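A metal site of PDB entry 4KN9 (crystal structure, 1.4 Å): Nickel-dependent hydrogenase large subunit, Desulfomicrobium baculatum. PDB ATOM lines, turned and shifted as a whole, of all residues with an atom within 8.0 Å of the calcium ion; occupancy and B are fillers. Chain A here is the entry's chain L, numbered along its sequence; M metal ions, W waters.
Three residues have an atom within 4 Å of the calcium ion: Glu 52, Ile 445 and His 499.
The nearest printed residue that does not touch the calcium ion is Glu 286 (4.2 Å).
The side-chain carboxylate (OE2) of Glu 52 lies within hydrogen-bond range of the side-chain hydroxyl (OG1) of Thr 308 (2.6 Å).
The backbone carbonyl oxygen (O) of Cys 496 sits at hydrogen-bond distance from a ring nitrogen (ND1) of His 499.
Water W2 lies within hydrogen-bond range of the side-chain carboxylate of Glu 286, the side-chain amide oxygen of Gln 444 and the side-chain amino group of Lys 322.
Water W3 lies within hydrogen-bond range of the side-chain carboxylate (OE2) of Glu 52 and the side-chain amino group (NZ) of Lys 322.
The calcium ion is bound by water W2.
The calcium ion is bound by water W3.
The calcium ion is bound by water W1 (2.3 Å).
O of Ile 445 binds the calcium ion (2.4 Å).
OE1 of Glu 52 binds the calcium ion (2.4 Å).
The calcium ion is bound by a ring nitrogen (NE2) of His 499.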
ATOM      1  N   PHE A  48       4.725  17.648  -3.541  1.00  0.00           N
ATOM      2  CA  PHE A  48       3.651  16.733  -3.880  1.00  0.00           C
ATOM      3  C   PHE A  48       2.435  17.546  -4.318  1.00  0.00           C
ATOM      4  O   PHE A  48       2.101  18.544  -3.662  1.00  0.00           O
ATOM      5  CB  PHE A  48       3.296  15.881  -2.654  1.00  0.00           C
ATOM      6  CG  PHE A  48       2.053  15.026  -2.818  1.00  0.00           C
ATOM      7  CD1 PHE A  48       2.107  13.818  -3.525  1.00  0.00           C
ATOM      8  CD2 PHE A  48       0.815  15.425  -2.277  1.00  0.00           C
ATOM      9  CE1 PHE A  48       0.960  13.021  -3.676  1.00  0.00           C
ATOM     10  CE2 PHE A  48      -0.319  14.633  -2.422  1.00  0.00           C
ATOM     11  CZ  PHE A  48      -0.246  13.418  -3.131  1.00  0.00           C
ATOM     12  N   GLU A  52      -3.270  11.881  -8.841  1.00  0.00           N
ATOM     13  CA  GLU A  52      -4.098  10.690  -8.792  1.00  0.00           C
ATOM     14  C   GLU A  52      -5.350  10.934  -7.927  1.00  0.00           C
ATOM     15  O   GLU A  52      -6.411  10.370  -8.202  1.00  0.00           O
ATOM     16  CB  GLU A  52      -3.294   9.493  -8.297  1.00  0.00           C
ATOM     17  CG  GLU A  52      -2.150   9.145  -9.261  1.00  0.00           C
ATOM     18  CD  GLU A  52      -0.986   8.442  -8.587  1.00  0.00           C
ATOM     19  OE1 GLU A  52      -0.320   7.598  -9.262  1.00  0.00           O
ATOM     20  OE2 GLU A  52      -0.703   8.721  -7.393  1.00  0.00           O
ATOM     21  N   GLU A 286       4.933  -1.129  -6.326  1.00  0.00           N
ATOM     22  CA  GLU A 286       5.470   0.032  -5.608  1.00  0.00           C
ATOM     23  C   GLU A 286       5.446  -0.213  -4.111  1.00  0.00           C
ATOM     24  O   GLU A 286       4.416  -0.601  -3.549  1.00  0.00           O
ATOM     25  CB  GLU A 286       4.658   1.274  -5.957  1.00  0.00           C
ATOM     26  CG  GLU A 286       4.837   1.705  -7.409  1.00  0.00           C
ATOM     27  CD  GLU A 286       4.033   2.933  -7.729  1.00  0.00           C
ATOM     28  OE1 GLU A 286       4.639   4.020  -7.839  1.00  0.00           O
ATOM     29  OE2 GLU A 286       2.785   2.823  -7.815  1.00  0.00           O
ATOM     30  N   PHE A 293       3.632   7.994   2.223  1.00  0.00           N
ATOM     31  CA  PHE A 293       2.351   7.405   1.808  1.00  0.00           C
ATOM     32  C   PHE A 293       1.946   6.237   2.685  1.00  0.00           C
ATOM     33  O   PHE A 293       2.818   5.523   3.189  1.00  0.00           O
ATOM     34  CB  PHE A 293       2.408   6.934   0.350  1.00  0.00           C
ATOM     35  CG  PHE A 293       2.558   8.058  -0.626  1.00  0.00           C
ATOM     36  CD1 PHE A 293       1.447   8.828  -0.998  1.00  0.00           C
ATOM     37  CD2 PHE A 293       3.817   8.396  -1.127  1.00  0.00           C
ATOM     38  CE1 PHE A 293       1.591   9.916  -1.862  1.00  0.00           C
ATOM     39  CE2 PHE A 293       3.956   9.471  -1.989  1.00  0.00           C
ATOM     40  CZ  PHE A 293       2.844  10.235  -2.353  1.00  0.00           C
ATOM     41  N   TYR A 303       0.312  -1.523  -9.641  1.00  0.00           N
ATOM     42  CA  TYR A 303      -0.310  -0.231  -9.963  1.00  0.00           C
ATOM     43  C   TYR A 303      -1.815  -0.348 -10.209  1.00  0.00           C
ATOM     44  O   TYR A 303      -2.538   0.627 -10.005  1.00  0.00           O
ATOM     45  CB  TYR A 303       0.394   0.430 -11.148  1.00  0.00           C
ATOM     46  CG  TYR A 303       0.369  -0.428 -12.382  1.00  0.00           C
ATOM     47  CD1 TYR A 303      -0.767  -0.451 -13.216  1.00  0.00           C
ATOM     48  CD2 TYR A 303       1.464  -1.199 -12.736  1.00  0.00           C
ATOM     49  CE1 TYR A 303      -0.797  -1.250 -14.356  1.00  0.00           C
ATOM     50  CE2 TYR A 303       1.443  -2.007 -13.868  1.00  0.00           C
ATOM     51  CZ  TYR A 303       0.319  -2.030 -14.675  1.00  0.00           C
ATOM     52  OH  TYR A 303       0.311  -2.832 -15.788  1.00  0.00           O
ATOM     53  N   GLY A 306      -3.198   0.432  -7.079  1.00  0.00           N
ATOM     54  CA  GLY A 306      -2.380   1.435  -6.409  1.00  0.00           C
ATOM     55  C   GLY A 306      -3.243   2.384  -5.581  1.00  0.00           C
ATOM     56  O   GLY A 306      -4.432   2.559  -5.859  1.00  0.00           O
ATOM     57  N   GLU A 307      -2.617   3.000  -4.583  1.00  0.00           N
ATOM     58  CA  GLU A 307      -3.304   3.851  -3.628  1.00  0.00           C
ATOM     59  C   GLU A 307      -2.456   5.083  -3.426  1.00  0.00           C
ATOM     60  O   GLU A 307      -1.228   4.986  -3.310  1.00  0.00           O
ATOM     61  CB  GLU A 307      -3.420   3.142  -2.283  1.00  0.00           C
ATOM     62  CG  GLU A 307      -4.379   1.952  -2.285  1.00  0.00           C
ATOM     63  CD  GLU A 307      -4.268   1.141  -0.995  1.00  0.00           C
ATOM     64  OE1 GLU A 307      -3.580   1.615  -0.053  1.00  0.00           O
ATOM     65  OE2 GLU A 307      -4.865   0.029  -0.940  1.00  0.00           O
ATOM     66  N   THR A 308      -3.114   6.226  -3.324  1.00  0.00           N
ATOM     67  CA  THR A 308      -2.432   7.497  -3.102  1.00  0.00           C
ATOM     68  C   THR A 308      -3.042   8.190  -1.882  1.00  0.00           C
ATOM     69  O   THR A 308      -3.986   8.989  -1.995  1.00  0.00           O
ATOM     70  CB  THR A 308      -2.467   8.367  -4.370  1.00  0.00           C
ATOM     71  OG1 THR A 308      -1.935   7.578  -5.437  1.00  0.00           O
ATOM     72  CG2 THR A 308      -1.619   9.632  -4.207  1.00  0.00           C
ATOM     73  N   PHE A 320       8.626  12.072  -1.138  1.00  0.00           N
ATOM     74  CA  PHE A 320       7.302  11.907  -1.775  1.00  0.00           C
ATOM     75  C   PHE A 320       7.315  10.971  -2.984  1.00  0.00           C
ATOM     76  O   PHE A 320       6.285  10.764  -3.618  1.00  0.00           O
ATOM     77  CB  PHE A 320       6.692  13.245  -2.175  1.00  0.00           C
ATOM     78  CG  PHE A 320       6.149  14.045  -1.000  1.00  0.00           C
ATOM     79  CD1 PHE A 320       5.007  13.615  -0.316  1.00  0.00           C
ATOM     80  CD2 PHE A 320       6.773  15.238  -0.609  1.00  0.00           C
ATOM     81  CE1 PHE A 320       4.497  14.345   0.762  1.00  0.00           C
ATOM     82  CE2 PHE A 320       6.263  15.968   0.470  1.00  0.00           C
ATOM     83  CZ  PHE A 320       5.137  15.525   1.161  1.00  0.00           C
ATOM     84  N   LYS A 322       7.433   7.325  -4.486  1.00  0.00           N
ATOM     85  CA  LYS A 322       7.271   5.893  -4.150  1.00  0.00           C
ATOM     86  C   LYS A 322       8.462   5.091  -4.661  1.00  0.00           C
ATOM     87  O   LYS A 322       9.300   5.629  -5.390  1.00  0.00           O
ATOM     88  CB  LYS A 322       5.959   5.329  -4.693  1.00  0.00           C
ATOM     89  CG  LYS A 322       4.700   6.028  -4.173  1.00  0.00           C
ATOM     90  CD  LYS A 322       3.460   5.262  -4.624  1.00  0.00           C
ATOM     91  CE  LYS A 322       2.155   5.898  -4.121  1.00  0.00           C
ATOM     92  NZ  LYS A 322       0.960   5.444  -4.950  1.00  0.00           N
ATOM     93  N   LEU A 430       3.809   4.386 -17.538  1.00  0.00           N
ATOM     94  CA  LEU A 430       2.460   3.869 -17.760  1.00  0.00           C
ATOM     95  C   LEU A 430       1.451   4.687 -16.998  1.00  0.00           C
ATOM     96  O   LEU A 430       1.766   5.256 -15.922  1.00  0.00           O
ATOM     97  CB  LEU A 430       2.349   2.373 -17.438  1.00  0.00           C
ATOM     98  CG  LEU A 430       2.490   1.914 -15.979  1.00  0.00           C
ATOM     99  CD1 LEU A 430       1.149   2.045 -15.230  1.00  0.00           C
ATOM    100  CD2 LEU A 430       3.025   0.488 -15.927  1.00  0.00           C
ATOM    101  N   TYR A 443      -6.883   6.270 -10.915  1.00  0.00           N
ATOM    102  CA  TYR A 443      -5.931   6.590 -11.962  1.00  0.00           C
ATOM    103  C   TYR A 443      -4.567   6.479 -11.308  1.00  0.00           C
ATOM    104  O   TYR A 443      -4.317   7.111 -10.274  1.00  0.00           O
ATOM    105  CB  TYR A 443      -6.182   8.004 -12.497  1.00  0.00           C
ATOM    106  CG  TYR A 443      -5.599   8.273 -13.874  1.00  0.00           C
ATOM    107  CD1 TYR A 443      -4.220   8.439 -14.049  1.00  0.00           C
ATOM    108  CD2 TYR A 443      -6.424   8.368 -14.987  1.00  0.00           C
ATOM    109  CE1 TYR A 443      -3.695   8.706 -15.312  1.00  0.00           C
ATOM    110  CE2 TYR A 443      -5.909   8.633 -16.242  1.00  0.00           C
ATOM    111  CZ  TYR A 443      -4.541   8.796 -16.408  1.00  0.00           C
ATOM    112  OH  TYR A 443      -4.067   9.066 -17.667  1.00  0.00           O
ATOM    113  N   GLN A 444      -3.694   5.661 -11.871  1.00  0.00           N
ATOM    114  CA  GLN A 444      -2.380   5.447 -11.266  1.00  0.00           C
ATOM    115  C   GLN A 444      -1.302   5.671 -12.309  1.00  0.00           C
ATOM    116  O   GLN A 444      -1.386   5.160 -13.422  1.00  0.00           O
ATOM    117  CB  GLN A 444      -2.270   4.041 -10.653  1.00  0.00           C
ATOM    118  CG  GLN A 444      -3.145   3.872  -9.400  1.00  0.00           C
ATOM    119  CD  GLN A 444      -2.627   4.657  -8.208  1.00  0.00           C
ATOM    120  OE1 GLN A 444      -1.449   4.557  -7.851  1.00  0.00           O
ATOM    121  NE2 GLN A 444      -3.504   5.421  -7.561  1.00  0.00           N
ATOM    122  N   ILE A 445      -0.308   6.476 -11.930  1.00  0.00           N
ATOM    123  CA  ILE A 445       0.778   6.875 -12.827  1.00  0.00           C
ATOM    124  C   ILE A 445       2.062   6.263 -12.287  1.00  0.00           C
ATOM    125  O   ILE A 445       2.372   6.441 -11.101  1.00  0.00           O
ATOM    126  CB  ILE A 445       0.863   8.399 -12.893  1.00  0.00           C
ATOM    127  CG1 ILE A 445      -0.426   8.955 -13.526  1.00  0.00           C
ATOM    128  CG2 ILE A 445       2.116   8.850 -13.640  1.00  0.00           C
ATOM    129  CD1 ILE A 445      -0.827  10.270 -13.038  1.00  0.00           C
ATOM    130  N   VAL A 446       2.793   5.545 -13.146  1.00  0.00           N
ATOM    131  CA  VAL A 446       4.113   5.009 -12.796  1.00  0.00           C
ATOM    132  C   VAL A 446       5.026   5.632 -13.826  1.00  0.00           C
ATOM    133  O   VAL A 446       5.037   5.217 -14.986  1.00  0.00           O
ATOM    134  CB  VAL A 446       4.115   3.474 -12.809  1.00  0.00           C
ATOM    135  CG1 VAL A 446       5.481   2.946 -12.443  1.00  0.00           C
ATOM    136  CG2 VAL A 446       3.039   2.944 -11.844  1.00  0.00           C
ATOM    137  N   SER A 447       5.795   6.629 -13.387  1.00  0.00           N
ATOM    138  CA  SER A 447       6.541   7.478 -14.294  1.00  0.00           C
ATOM    139  C   SER A 447       8.023   7.105 -14.333  1.00  0.00           C
ATOM    140  O   SER A 447       8.508   6.300 -13.545  1.00  0.00           O
ATOM    141  CB  SER A 447       6.393   8.946 -13.867  1.00  0.00           C
ATOM    142  OG  SER A 447       6.992   9.116 -12.601  1.00  0.00           O
ATOM    143  N   LEU A 450      10.341   8.299 -11.411  1.00  0.00           N
ATOM    144  CA  LEU A 450       9.906   7.452 -10.299  1.00  0.00           C
ATOM    145  C   LEU A 450      10.820   6.211 -10.182  1.00  0.00           C
ATOM    146  O   LEU A 450      11.196   5.843  -9.062  1.00  0.00           O
ATOM    147  CB  LEU A 450       8.464   7.005 -10.526  1.00  0.00           C
ATOM    148  CG  LEU A 450       7.941   5.914  -9.602  1.00  0.00           C
ATOM    149  CD1 LEU A 450       7.723   6.416  -8.167  1.00  0.00           C
ATOM    150  CD2 LEU A 450       6.641   5.418 -10.167  1.00  0.00           C
ATOM    151  N   CYS A 496       7.379  14.700 -12.404  1.00  0.00           N
ATOM    152  CA  CYS A 496       6.940  13.376 -12.844  1.00  0.00           C
ATOM    153  C   CYS A 496       7.078  12.328 -11.790  1.00  0.00           C
ATOM    154  O   CYS A 496       6.219  11.457 -11.684  1.00  0.00           O
ATOM    155  CB  CYS A 496       7.717  12.877 -14.036  1.00  0.00           C
ATOM    156  SG  CYS A 496       7.403  13.814 -15.539  1.00  0.00           S
ATOM    157  N   ALA A 497       8.164  12.398 -11.020  1.00  0.00           N
ATOM    158  CA  ALA A 497       8.455  11.315 -10.050  1.00  0.00           C
ATOM    159  C   ALA A 497       7.343  11.233  -8.996  1.00  0.00           C
ATOM    160  O   ALA A 497       7.002  10.143  -8.555  1.00  0.00           O
ATOM    161  CB  ALA A 497       9.815  11.513  -9.354  1.00  0.00           C
ATOM    162  N   VAL A 498       6.806  12.395  -8.600  1.00  0.00           N
ATOM    163  CA  VAL A 498       5.877  12.479  -7.459  1.00  0.00           C
ATOM    164  C   VAL A 498       4.432  12.654  -7.904  1.00  0.00           C
ATOM    165  O   VAL A 498       3.539  12.022  -7.346  1.00  0.00           O
ATOM    166  CB  VAL A 498       6.238  13.642  -6.510  1.00  0.00           C
ATOM    167  CG1 VAL A 498       5.192  13.729  -5.379  1.00  0.00           C
ATOM    168  CG2 VAL A 498       7.657  13.492  -5.951  1.00  0.00           C
ATOM    169  N   HIS A 499       4.214  13.503  -8.909  1.00  0.00           N
ATOM    170  CA  HIS A 499       2.896  13.865  -9.427  1.00  0.00           C
ATOM    171  C   HIS A 499       1.921  14.122  -8.306  1.00  0.00           C
ATOM    172  O   HIS A 499       0.807  13.593  -8.286  1.00  0.00           O
ATOM    173  CB  HIS A 499       2.365  12.874 -10.498  1.00  0.00           C
ATOM    174  CG  HIS A 499       2.608  11.418 -10.186  1.00  0.00           C
ATOM    175  ND1 HIS A 499       3.823  10.806 -10.396  1.00  0.00           N
ATOM    176  CD2 HIS A 499       1.796  10.478  -9.627  1.00  0.00           C
ATOM    177  CE1 HIS A 499       3.756   9.544 -10.016  1.00  0.00           C
ATOM    178  NE2 HIS A 499       2.548   9.322  -9.531  1.00  0.00           N
HETATM  179 CA    CA M   1       1.941   7.035  -8.853  1.00  0.00          CA
HETATM  180  O   HOH W   1       4.094   6.528  -8.131  1.00  0.00           O
HETATM  181  O   HOH W   2       1.353   4.972  -8.306  1.00  0.00           O
HETATM  182  O   HOH W   3       1.723   7.869  -6.786  1.00  0.00           O
